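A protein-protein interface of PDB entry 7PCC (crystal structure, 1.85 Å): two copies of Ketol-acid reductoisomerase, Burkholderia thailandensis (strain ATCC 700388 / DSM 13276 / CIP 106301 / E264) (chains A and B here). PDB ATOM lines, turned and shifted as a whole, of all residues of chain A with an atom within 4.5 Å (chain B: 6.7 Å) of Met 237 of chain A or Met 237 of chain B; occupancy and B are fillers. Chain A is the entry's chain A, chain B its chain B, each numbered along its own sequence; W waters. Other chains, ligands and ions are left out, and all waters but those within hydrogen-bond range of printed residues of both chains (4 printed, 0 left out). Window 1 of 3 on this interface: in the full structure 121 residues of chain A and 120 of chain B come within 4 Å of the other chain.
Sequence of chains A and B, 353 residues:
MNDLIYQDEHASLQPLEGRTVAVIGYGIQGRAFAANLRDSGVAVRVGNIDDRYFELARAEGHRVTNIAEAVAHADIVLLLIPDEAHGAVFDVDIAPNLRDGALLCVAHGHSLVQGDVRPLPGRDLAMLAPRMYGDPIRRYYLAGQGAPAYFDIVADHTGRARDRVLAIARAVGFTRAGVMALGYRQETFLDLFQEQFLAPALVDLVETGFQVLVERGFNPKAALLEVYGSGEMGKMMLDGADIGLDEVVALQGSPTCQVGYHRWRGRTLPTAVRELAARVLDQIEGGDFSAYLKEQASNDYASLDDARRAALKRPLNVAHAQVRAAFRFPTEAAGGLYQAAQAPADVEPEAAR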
ATOM      1  N   VAL A 206      20.125  17.464  15.748  1.00  0.00           N
ATOM      2  CA  VAL A 206      18.973  18.409  15.693  1.00  0.00           C
ATOM      3  C   VAL A 206      18.013  18.056  16.835  1.00  0.00           C
ATOM      4  O   VAL A 206      17.623  18.965  17.602  1.00  0.00           O
ATOM      5  CB  VAL A 206      18.286  18.343  14.316  1.00  0.00           C
ATOM      6  CG1 VAL A 206      16.892  18.941  14.334  1.00  0.00           C
ATOM      7  CG2 VAL A 206      19.140  19.003  13.248  1.00  0.00           C
ATOM      8  N   TYR A 228      15.941  23.296  13.175  1.00  0.00           N
ATOM      9  CA  TYR A 228      15.826  23.036  11.713  1.00  0.00           C
ATOM     10  C   TYR A 228      14.546  23.612  11.102  1.00  0.00           C
ATOM     11  O   TYR A 228      14.569  23.823   9.880  1.00  0.00           O
ATOM     12  CB  TYR A 228      15.870  21.536  11.404  1.00  0.00           C
ATOM     13  CG  TYR A 228      14.569  20.809  11.629  1.00  0.00           C
ATOM     14  CD1 TYR A 228      14.219  20.348  12.885  1.00  0.00           C
ATOM     15  CD2 TYR A 228      13.686  20.581  10.587  1.00  0.00           C
ATOM     16  CE1 TYR A 228      13.029  19.679  13.105  1.00  0.00           C
ATOM     17  CE2 TYR A 228      12.486  19.920  10.790  1.00  0.00           C
ATOM     18  CZ  TYR A 228      12.157  19.466  12.053  1.00  0.00           C
ATOM     19  OH  TYR A 228      10.980  18.821  12.269  1.00  0.00           O
ATOM     20  N   MET A 233      19.128  26.043   9.282  1.00  0.00           N
ATOM     21  CA  MET A 233      20.213  25.026   9.305  1.00  0.00           C
ATOM     22  C   MET A 233      20.299  24.351   7.930  1.00  0.00           C
ATOM     23  O   MET A 233      21.426  24.152   7.449  1.00  0.00           O
ATOM     24  CB  MET A 233      20.002  23.988  10.412  1.00  0.00           C
ATOM     25  CG  MET A 233      20.161  24.554  11.823  1.00  0.00           C
ATOM     26  SD  MET A 233      21.826  25.179  12.204  1.00  0.00           S
ATOM     27  CE  MET A 233      21.649  26.906  11.761  1.00  0.00           C
ATOM     28  N   GLY A 234      19.158  24.062   7.300  1.00  0.00           N
ATOM     29  CA  GLY A 234      19.087  23.539   5.922  1.00  0.00           C
ATOM     30  C   GLY A 234      19.705  24.495   4.913  1.00  0.00           C
ATOM     31  O   GLY A 234      20.481  24.028   4.056  1.00  0.00           O
ATOM     32  N   LYS A 235      19.385  25.789   5.004  1.00  0.00           N
ATOM     33  CA  LYS A 235      19.947  26.836   4.109  1.00  0.00           C
ATOM     34  C   LYS A 235      21.464  26.917   4.313  1.00  0.00           C
ATOM     35  O   LYS A 235      22.182  26.971   3.316  1.00  0.00           O
ATOM     36  CB  LYS A 235      19.288  28.196   4.359  1.00  0.00           C
ATOM     37  CG  LYS A 235      17.855  28.327   3.854  1.00  0.00           C
ATOM     38  CD  LYS A 235      17.702  28.157   2.354  1.00  0.00           C
ATOM     39  CE  LYS A 235      18.114  29.377   1.564  1.00  0.00           C
ATOM     40  NZ  LYS A 235      17.968  29.140   0.108  1.00  0.00           N
ATOM     41  N   MET A 236      21.932  26.909   5.563  1.00  0.00           N
ATOM     42  CA  MET A 236      23.384  26.952   5.887  1.00  0.00           C
ATOM     43  C   MET A 236      24.095  25.767   5.218  1.00  0.00           C
ATOM     44  O   MET A 236      25.174  25.974   4.632  1.00  0.00           O
ATOM     45  CB  MET A 236      23.618  26.897   7.399  1.00  0.00           C
ATOM     46  CG  MET A 236      25.080  27.025   7.780  1.00  0.00           C
ATOM     47  SD  MET A 236      25.362  26.597   9.501  1.00  0.00           S
ATOM     48  CE  MET A 236      25.243  24.811   9.413  1.00  0.00           C
ATOM     49  N   MET A 237      23.510  24.571   5.306  1.00  0.00           N
ATOM     50  CA  MET A 237      24.100  23.315   4.769  1.00  0.00           C
ATOM     51  C   MET A 237      24.097  23.338   3.234  1.00  0.00           C
ATOM     52  O   MET A 237      25.090  22.870   2.639  1.00  0.00           O
ATOM     53  CB  MET A 237      23.320  22.098   5.269  1.00  0.00           C
ATOM     54  CG  MET A 237      23.498  21.847   6.752  1.00  0.00           C
ATOM     55  SD  MET A 237      23.891  20.131   7.120  1.00  0.00           S
ATOM     56  CE  MET A 237      25.440  19.965   6.235  1.00  0.00           C
ATOM     57  N   LEU A 238      23.034  23.854   2.612  1.00  0.00           N
ATOM     58  CA  LEU A 238      22.883  23.874   1.130  1.00  0.00           C
ATOM     59  C   LEU A 238      23.737  25.002   0.533  1.00  0.00           C
ATOM     60  O   LEU A 238      24.387  24.758  -0.500  1.00  0.00           O
ATOM     61  CB  LEU A 238      21.406  24.023   0.745  1.00  0.00           C
ATOM     62  CG  LEU A 238      21.117  23.967  -0.755  1.00  0.00           C
ATOM     63  CD1 LEU A 238      21.548  22.634  -1.354  1.00  0.00           C
ATOM     64  CD2 LEU A 238      19.643  24.225  -1.036  1.00  0.00           C
ATOM     65  N   ASP A 239      23.738  26.188   1.147  1.00  0.00           N
ATOM     66  CA  ASP A 239      24.652  27.296   0.753  1.00  0.00           C
ATOM     67  C   ASP A 239      26.096  26.843   0.999  1.00  0.00           C
ATOM     68  O   ASP A 239      26.972  27.203   0.191  1.00  0.00           O
ATOM     69  CB  ASP A 239      24.348  28.595   1.502  1.00  0.00           C
ATOM     70  CG  ASP A 239      23.081  29.290   1.043  1.00  0.00           C
ATOM     71  OD1 ASP A 239      22.567  28.924  -0.033  1.00  0.00           O
ATOM     72  OD2 ASP A 239      22.625  30.199   1.764  1.00  0.00           O
ATOM     73  N   GLY A 240      26.321  26.075   2.068  1.00  0.00           N
ATOM     74  CA  GLY A 240      27.638  25.507   2.420  1.00  0.00           C
ATOM     75  C   GLY A 240      28.177  24.610   1.320  1.00  0.00           C
ATOM     76  O   GLY A 240      29.388  24.665   1.051  1.00  0.00           O
ATOM     77  N   ALA A 241      27.312  23.807   0.693  1.00  0.00           N
ATOM     78  CA  ALA A 241      27.669  22.943  -0.458  1.00  0.00           C
ATOM     79  C   ALA A 241      28.309  23.807  -1.554  1.00  0.00           C
ATOM     80  O   ALA A 241      29.256  23.328  -2.215  1.00  0.00           O
ATOM     81  CB  ALA A 241      26.453  22.210  -0.964  1.00  0.00           C
ATOM     82  N   LEU A 245      31.141  25.379   4.417  1.00  0.00           N
ATOM     83  CA  LEU A 245      30.340  25.529   5.663  1.00  0.00           C
ATOM     84  C   LEU A 245      30.932  26.642   6.544  1.00  0.00           C
ATOM     85  O   LEU A 245      30.162  27.522   6.968  1.00  0.00           O
ATOM     86  CB  LEU A 245      30.279  24.178   6.380  1.00  0.00           C
ATOM     87  CG  LEU A 245      29.406  23.133   5.684  1.00  0.00           C
ATOM     88  CD1 LEU A 245      29.729  21.733   6.176  1.00  0.00           C
ATOM     89  CD2 LEU A 245      27.927  23.444   5.873  1.00  0.00           C
ATOM     90  N   TYR B 133      19.027  34.409   7.803  1.00  0.00           N
ATOM     91  CA  TYR B 133      20.006  35.426   7.343  1.00  0.00           C
ATOM     92  C   TYR B 133      19.434  36.125   6.101  1.00  0.00           C
ATOM     93  O   TYR B 133      18.313  35.787   5.670  1.00  0.00           O
ATOM     94  CB  TYR B 133      21.416  34.848   7.170  1.00  0.00           C
ATOM     95  CG  TYR B 133      21.583  33.574   6.377  1.00  0.00           C
ATOM     96  CD1 TYR B 133      21.466  32.338   6.991  1.00  0.00           C
ATOM     97  CD2 TYR B 133      21.972  33.594   5.047  1.00  0.00           C
ATOM     98  CE1 TYR B 133      21.666  31.158   6.294  1.00  0.00           C
ATOM     99  CE2 TYR B 133      22.174  32.424   4.330  1.00  0.00           C
ATOM    100  CZ  TYR B 133      22.026  31.200   4.958  1.00  0.00           C
ATOM    101  OH  TYR B 133      22.224  30.032   4.280  1.00  0.00           O
ATOM    102  N   LEU B 202      26.832  20.346  13.904  1.00  0.00           N
ATOM    103  CA  LEU B 202      26.422  19.864  12.557  1.00  0.00           C
ATOM    104  C   LEU B 202      27.646  19.855  11.635  1.00  0.00           C
ATOM    105  O   LEU B 202      27.865  18.826  10.969  1.00  0.00           O
ATOM    106  CB  LEU B 202      25.305  20.743  11.988  1.00  0.00           C
ATOM    107  CG  LEU B 202      23.919  20.555  12.604  1.00  0.00           C
ATOM    108  CD1 LEU B 202      22.926  21.523  11.985  1.00  0.00           C
ATOM    109  CD2 LEU B 202      23.421  19.125  12.449  1.00  0.00           C
ATOM    110  N   VAL B 203      28.419  20.946  11.617  1.00  0.00           N
ATOM    111  CA  VAL B 203      29.645  21.076  10.775  1.00  0.00           C
ATOM    112  C   VAL B 203      30.708  20.105  11.304  1.00  0.00           C
ATOM    113  O   VAL B 203      31.366  19.455  10.469  1.00  0.00           O
ATOM    114  CB  VAL B 203      30.157  22.528  10.702  1.00  0.00           C
ATOM    115  CG1 VAL B 203      31.414  22.640   9.851  1.00  0.00           C
ATOM    116  CG2 VAL B 203      29.083  23.473  10.174  1.00  0.00           C
ATOM    117  N   VAL B 206      29.611  16.657   9.995  1.00  0.00           N
ATOM    118  CA  VAL B 206      29.952  16.611   8.541  1.00  0.00           C
ATOM    119  C   VAL B 206      31.460  16.364   8.403  1.00  0.00           C
ATOM    120  O   VAL B 206      31.852  15.482   7.610  1.00  0.00           O
ATOM    121  CB  VAL B 206      29.523  17.907   7.829  1.00  0.00           C
ATOM    122  CG1 VAL B 206      30.163  18.048   6.459  1.00  0.00           C
ATOM    123  CG2 VAL B 206      28.012  18.008   7.719  1.00  0.00           C
ATOM    124  N   VAL B 227      29.136  14.064   2.180  1.00  0.00           N
ATOM    125  CA  VAL B 227      28.902  14.605   3.552  1.00  0.00           C
ATOM    126  C   VAL B 227      28.235  15.987   3.488  1.00  0.00           C
ATOM    127  O   VAL B 227      27.621  16.358   4.500  1.00  0.00           O
ATOM    128  CB  VAL B 227      30.170  14.591   4.428  1.00  0.00           C
ATOM    129  CG1 VAL B 227      30.678  13.169   4.612  1.00  0.00           C
ATOM    130  CG2 VAL B 227      31.269  15.507   3.906  1.00  0.00           C
ATOM    131  N   TYR B 228      28.308  16.708   2.358  1.00  0.00           N
ATOM    132  CA  TYR B 228      27.532  17.963   2.141  1.00  0.00           C
ATOM    133  C   TYR B 228      27.722  18.541   0.732  1.00  0.00           C
ATOM    134  O   TYR B 228      26.776  19.196   0.264  1.00  0.00           O
ATOM    135  CB  TYR B 228      27.886  19.033   3.178  1.00  0.00           C
ATOM    136  CG  TYR B 228      29.173  19.772   2.914  1.00  0.00           C
ATOM    137  CD1 TYR B 228      30.385  19.248   3.323  1.00  0.00           C
ATOM    138  CD2 TYR B 228      29.184  20.987   2.250  1.00  0.00           C
ATOM    139  CE1 TYR B 228      31.577  19.912   3.093  1.00  0.00           C
ATOM    140  CE2 TYR B 228      30.370  21.664   2.003  1.00  0.00           C
ATOM    141  CZ  TYR B 228      31.569  21.125   2.432  1.00  0.00           C
ATOM    142  OH  TYR B 228      32.751  21.764   2.200  1.00  0.00           O
ATOM    143  N   GLY B 229      28.889  18.340   0.105  1.00  0.00           N
ATOM    144  CA  GLY B 229      29.327  19.031  -1.124  1.00  0.00           C
ATOM    145  C   GLY B 229      28.381  18.844  -2.301  1.00  0.00           C
ATOM    146  O   GLY B 229      28.312  19.757  -3.142  1.00  0.00           O
ATOM    147  N   GLY B 231      25.207  18.799  -2.043  1.00  0.00           N
ATOM    148  CA  GLY B 231      23.994  19.552  -1.666  1.00  0.00           C
ATOM    149  C   GLY B 231      22.895  18.639  -1.145  1.00  0.00           C
ATOM    150  O   GLY B 231      21.837  19.158  -0.758  1.00  0.00           O
ATOM    151  N   GLU B 232      23.132  17.324  -1.120  1.00  0.00           N
ATOM    152  CA  GLU B 232      22.103  16.307  -0.777  1.00  0.00           C
ATOM    153  C   GLU B 232      21.708  16.440   0.698  1.00  0.00           C
ATOM    154  O   GLU B 232      20.500  16.452   0.978  1.00  0.00           O
ATOM    155  CB  GLU B 232      22.609  14.900  -1.094  1.00  0.00           C
ATOM    156  CG  GLU B 232      21.538  13.833  -0.971  1.00  0.00           C
ATOM    157  CD  GLU B 232      21.876  12.524  -1.663  1.00  0.00           C
ATOM    158  OE1 GLU B 232      23.053  12.120  -1.614  1.00  0.00           O
ATOM    159  OE2 GLU B 232      20.962  11.914  -2.255  1.00  0.00           O
ATOM    160  N   MET B 233      22.675  16.540   1.612  1.00  0.00           N
ATOM    161  CA  MET B 233      22.379  16.672   3.067  1.00  0.00           C
ATOM    162  C   MET B 233      21.684  18.016   3.312  1.00  0.00           C
ATOM    163  O   MET B 233      20.732  18.043   4.110  1.00  0.00           O
ATOM    164  CB  MET B 233      23.643  16.555   3.922  1.00  0.00           C
ATOM    165  CG  MET B 233      24.259  15.163   3.905  1.00  0.00           C
ATOM    166  SD  MET B 233      23.205  13.866   4.619  1.00  0.00           S
ATOM    167  CE  MET B 233      22.356  13.265   3.160  1.00  0.00           C
ATOM    168  N   GLY B 234      22.117  19.074   2.623  1.00  0.00           N
ATOM    169  CA  GLY B 234      21.471  20.400   2.652  1.00  0.00           C
ATOM    170  C   GLY B 234      20.021  20.327   2.203  1.00  0.00           C
ATOM    171  O   GLY B 234      19.155  20.874   2.910  1.00  0.00           O
ATOM    172  N   LYS B 235      19.758  19.656   1.078  1.00  0.00           N
ATOM    173  CA  LYS B 235      18.387  19.470   0.530  1.00  0.00           C
ATOM    174  C   LYS B 235      17.545  18.676   1.532  1.00  0.00           C
ATOM    175  O   LYS B 235      16.401  19.081   1.780  1.00  0.00           O
ATOM    176  CB  LYS B 235      18.417  18.769  -0.833  1.00  0.00           C
ATOM    177  CG  LYS B 235      18.906  19.617  -1.999  1.00  0.00           C
ATOM    178  CD  LYS B 235      18.069  20.848  -2.282  1.00  0.00           C
ATOM    179  CE  LYS B 235      16.856  20.573  -3.140  1.00  0.00           C
ATOM    180  NZ  LYS B 235      16.225  21.836  -3.593  1.00  0.00           N
ATOM    181  N   MET B 236      18.091  17.590   2.092  1.00  0.00           N
ATOM    182  CA  MET B 236      17.388  16.752   3.100  1.00  0.00           C
ATOM    183  C   MET B 236      16.945  17.631   4.279  1.00  0.00           C
ATOM    184  O   MET B 236      15.791  17.493   4.725  1.00  0.00           O
ATOM    185  CB  MET B 236      18.290  15.634   3.628  1.00  0.00           C
ATOM    186  CG  MET B 236      17.567  14.688   4.560  1.00  0.00           C
ATOM    187  SD  MET B 236      18.678  13.568   5.417  1.00  0.00           S
ATOM    188  CE  MET B 236      19.495  14.704   6.537  1.00  0.00           C
ATOM    189  N   MET B 237      17.846  18.482   4.775  1.00  0.00           N
ATOM    190  CA  MET B 237      17.606  19.347   5.958  1.00  0.00           C
ATOM    191  C   MET B 237      16.613  20.463   5.603  1.00  0.00           C
ATOM    192  O   MET B 237      15.810  20.821   6.474  1.00  0.00           O
ATOM    193  CB  MET B 237      18.921  19.938   6.466  1.00  0.00           C
ATOM    194  CG  MET B 237      19.852  18.877   7.020  1.00  0.00           C
ATOM    195  SD  MET B 237      20.816  19.431   8.436  1.00  0.00           S
ATOM    196  CE  MET B 237      19.513  19.738   9.627  1.00  0.00           C
ATOM    197  N   LEU B 238      16.650  20.978   4.373  1.00  0.00           N
ATOM    198  CA  LEU B 238      15.749  22.071   3.919  1.00  0.00           C
ATOM    199  C   LEU B 238      14.361  21.491   3.628  1.00  0.00           C
ATOM    200  O   LEU B 238      13.380  22.045   4.138  1.00  0.00           O
ATOM    201  CB  LEU B 238      16.349  22.758   2.688  1.00  0.00           C
ATOM    202  CG  LEU B 238      15.727  24.099   2.300  1.00  0.00           C
ATOM    203  CD1 LEU B 238      15.701  25.063   3.479  1.00  0.00           C
ATOM    204  CD2 LEU B 238      16.477  24.719   1.126  1.00  0.00           C
ATOM    205  N   ASP B 239      14.284  20.406   2.851  1.00  0.00           N
ATOM    206  CA  ASP B 239      13.013  19.671   2.604  1.00  0.00           C
ATOM    207  C   ASP B 239      12.453  19.202   3.951  1.00  0.00           C
ATOM    208  O   ASP B 239      11.225  19.264   4.126  1.00  0.00           O
ATOM    209  CB  ASP B 239      13.203  18.498   1.637  1.00  0.00           C
ATOM    210  CG  ASP B 239      13.395  18.923   0.192  1.00  0.00           C
ATOM    211  OD1 ASP B 239      13.254  20.129  -0.087  1.00  0.00           O
ATOM    212  OD2 ASP B 239      13.689  18.042  -0.642  1.00  0.00           O
ATOM    213  N   GLY B 240      13.329  18.775   4.866  1.00  0.00           N
ATOM    214  CA  GLY B 240      12.968  18.349   6.234  1.00  0.00           C
ATOM    215  C   GLY B 240      12.255  19.445   7.010  1.00  0.00           C
ATOM    216  O   GLY B 240      11.290  19.129   7.727  1.00  0.00           O
ATOM    217  N   ALA B 241      12.708  20.694   6.883  1.00  0.00           N
ATOM    218  CA  ALA B 241      12.071  21.864   7.531  1.00  0.00           C
ATOM    219  C   ALA B 241      10.606  21.941   7.087  1.00  0.00           C
ATOM    220  O   ALA B 241       9.752  22.250   7.934  1.00  0.00           O
ATOM    221  CB  ALA B 241      12.827  23.127   7.208  1.00  0.00           C
ATOM    222  N   ASP B 242      10.325  21.635   5.816  1.00  0.00           N
ATOM    223  CA  ASP B 242       8.949  21.642   5.251  1.00  0.00           C
ATOM    224  C   ASP B 242       8.142  20.485   5.855  1.00  0.00           C
ATOM    225  O   ASP B 242       7.177  20.769   6.589  1.00  0.00           O
ATOM    226  CB  ASP B 242       8.962  21.565   3.722  1.00  0.00           C
ATOM    227  CG  ASP B 242       7.579  21.685   3.099  1.00  0.00           C
ATOM    228  OD1 ASP B 242       6.658  22.147   3.800  1.00  0.00           O
ATOM    229  OD2 ASP B 242       7.433  21.306   1.920  1.00  0.00           O
ATOM    230  N   LEU B 245      12.020  15.759   9.118  1.00  0.00           N
ATOM    231  CA  LEU B 245      13.321  15.131   8.758  1.00  0.00           C
ATOM    232  C   LEU B 245      13.138  13.622   8.546  1.00  0.00           C
ATOM    233  O   LEU B 245      13.657  13.104   7.545  1.00  0.00           O
ATOM    234  CB  LEU B 245      14.352  15.430   9.850  1.00  0.00           C
ATOM    235  CG  LEU B 245      14.926  16.845   9.828  1.00  0.00           C
ATOM    236  CD1 LEU B 245      15.662  17.159  11.122  1.00  0.00           C
ATOM    237  CD2 LEU B 245      15.847  17.035   8.630  1.00  0.00           C
ATOM    238  N   VAL B 248      11.179  13.094   5.233  1.00  0.00           N
ATOM    239  CA  VAL B 248      12.025  13.246   4.010  1.00  0.00           C
ATOM    240  C   VAL B 248      12.592  11.876   3.627  1.00  0.00           C
ATOM    241  O   VAL B 248      12.582  11.544   2.431  1.00  0.00           O
ATOM    242  CB  VAL B 248      13.150  14.282   4.209  1.00  0.00           C
ATOM    243  CG1 VAL B 248      14.267  14.115   3.193  1.00  0.00           C
ATOM    244  CG2 VAL B 248      12.606  15.697   4.158  1.00  0.00           C
ATOM    245  N   PHE B 329      28.126  23.782  -9.461  1.00  0.00           N
ATOM    246  CA  PHE B 329      27.023  23.719  -8.468  1.00  0.00           C
ATOM    247  C   PHE B 329      25.843  24.555  -8.954  1.00  0.00           C
ATOM    248  O   PHE B 329      26.032  25.665  -9.440  1.00  0.00           O
ATOM    249  CB  PHE B 329      27.496  24.187  -7.093  1.00  0.00           C
ATOM    250  CG  PHE B 329      26.553  23.794  -5.987  1.00  0.00           C
ATOM    251  CD1 PHE B 329      25.607  24.688  -5.509  1.00  0.00           C
ATOM    252  CD2 PHE B 329      26.566  22.507  -5.473  1.00  0.00           C
ATOM    253  CE1 PHE B 329      24.719  24.314  -4.512  1.00  0.00           C
ATOM    254  CE2 PHE B 329      25.679  22.136  -4.474  1.00  0.00           C
ATOM    255  CZ  PHE B 329      24.759  23.039  -3.995  1.00  0.00           C
HETATM  256  O   HOH W   1      33.096  23.245   4.185  1.00  0.00           O
HETATM  257  O   HOH W   2      24.605  20.153   1.704  1.00  0.00           O
HETATM  258  O   HOH W   3      11.567  16.417  11.878  1.00  0.00           O
HETATM  259  O   HOH W   4      16.516  23.186   8.001  1.00  0.00           O
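CE of Met 237 of chain B touches CG2 of Val 206 of chain A, at 3.7 Å. Ala 241 of chain B touches Tyr 228 of chain A. Met 233 of chain A touches Leu 202 of chain B. Gly 234 of chain A touches Met 237 of chain B (CA to CB, 3.6 Å). Gly 234 of chain A touches Leu 238 of chain B. Leu 238 of chain A touches Gly 231 of chain B. CD2 of Leu 238 of chain A touches CD2 of Leu 238 of chain B (3.9 Å). Phe 329 of chain B touches Leu 238 of chain A. Leu 245 of chain A touches Val 203 of chain B (CB to CG1, 3.96 Å). Leu 245 of chain A touches Val 206 of chain B.
Of the printed residues of chain B, Val 206 of chain A touches Met 237 and Leu 245. Of chain B, only Val 206, Gly 234 and Met 237 come within 4 Å of Met 237 of chain A. Of the printed residues of chain B, Leu 245 of chain A touches Val 203, Val 206 and Tyr 228. Of the printed residues of chain A, Val 206 of chain B touches Met 237 (3.6 Å) and Leu 245 (3.7 Å). Met 236 of chain B touches none of the printed residues of chain A. Of chain A, only Val 206 (3.7 Å), Gly 234 (3.6 Å) and Met 237 (3.4 Å) come within 4 Å of Met 237 of chain B. Asp 239 of chain B touches none of the printed residues of chain A. Printed residues of chain A within 4 Å of Leu 245 of chain B: Val 206 and Tyr 228. The nearest residue of chain B that does not touch Met 237 of chain A is Tyr 228 of chain B (4.02 Å). The nearest printed residue of chain A that does not touch Gly 231 of chain B is Met 237 of chain A (5.5 Å).
Hydrophobic or aromatic side chains of chain B within 4 Å of the printed part of chain A: Tyr 133, Leu 202, Val 203, Val 206, Tyr 228, Met 237, Leu 238, Ala 241, Leu 245 and Phe 329. Of the 12 printed residues of chain A, 12 touch a printed residue of chain B.
Water W1 bridges OH of Tyr 228 of chain B and N of Leu 245 of chain A. Water W3 bridges OH of Tyr 228 of chain A and N of Leu 245 of chain B. Water W2 lies within hydrogen-bond range of O of Tyr 228 of chain B (2.8 Å), N of Gly 234 of chain B (2.9 Å) and O of Met 237 of chain A (2.9 Å). Water W4 lies within hydrogen-bond range of the backbone carbonyl oxygen of Tyr 228 of chain A, the backbone NH of Gly 234 of chain A and the backbone carbonyl oxygen of Met 237 of chain B.
Val 206 of chain A touches Met 237 of chain B, and with the chains exchanged Met 237 of chain A touches Val 206 of chain B. Gly 234 of chain A touches Met 237 of chain B, and with the chains exchanged Met 237 of chain A touches Gly 234 of chain B. Gly 234 of chain A touches Leu 238 of chain B, and with the chains exchanged Leu 238 of chain A touches Gly 234 of chain B. Leu 238 of chain A touches its own counterpart, Leu 238 of chain B. 12 positions are printed for both chains.
The backbone carbonyl oxygen (O) of Lys 235 of chain A lies close to the side-chain hydroxyl (OH) of Tyr 133 of chain B, at 3.2 Å. The backbone NH (N) of Met 236 of chain A sits at hydrogen-bond distance from the side-chain hydroxyl (OH) of Tyr 133 of chain B, at 3.4 Å. OD2 of Asp 239 of chain A lies within hydrogen-bond range of OH of Tyr 133 of chain B, at 2.6 Å. SD of Met 237 of chain A lies close to SD of Met 237 of chain B (3.4 Å).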
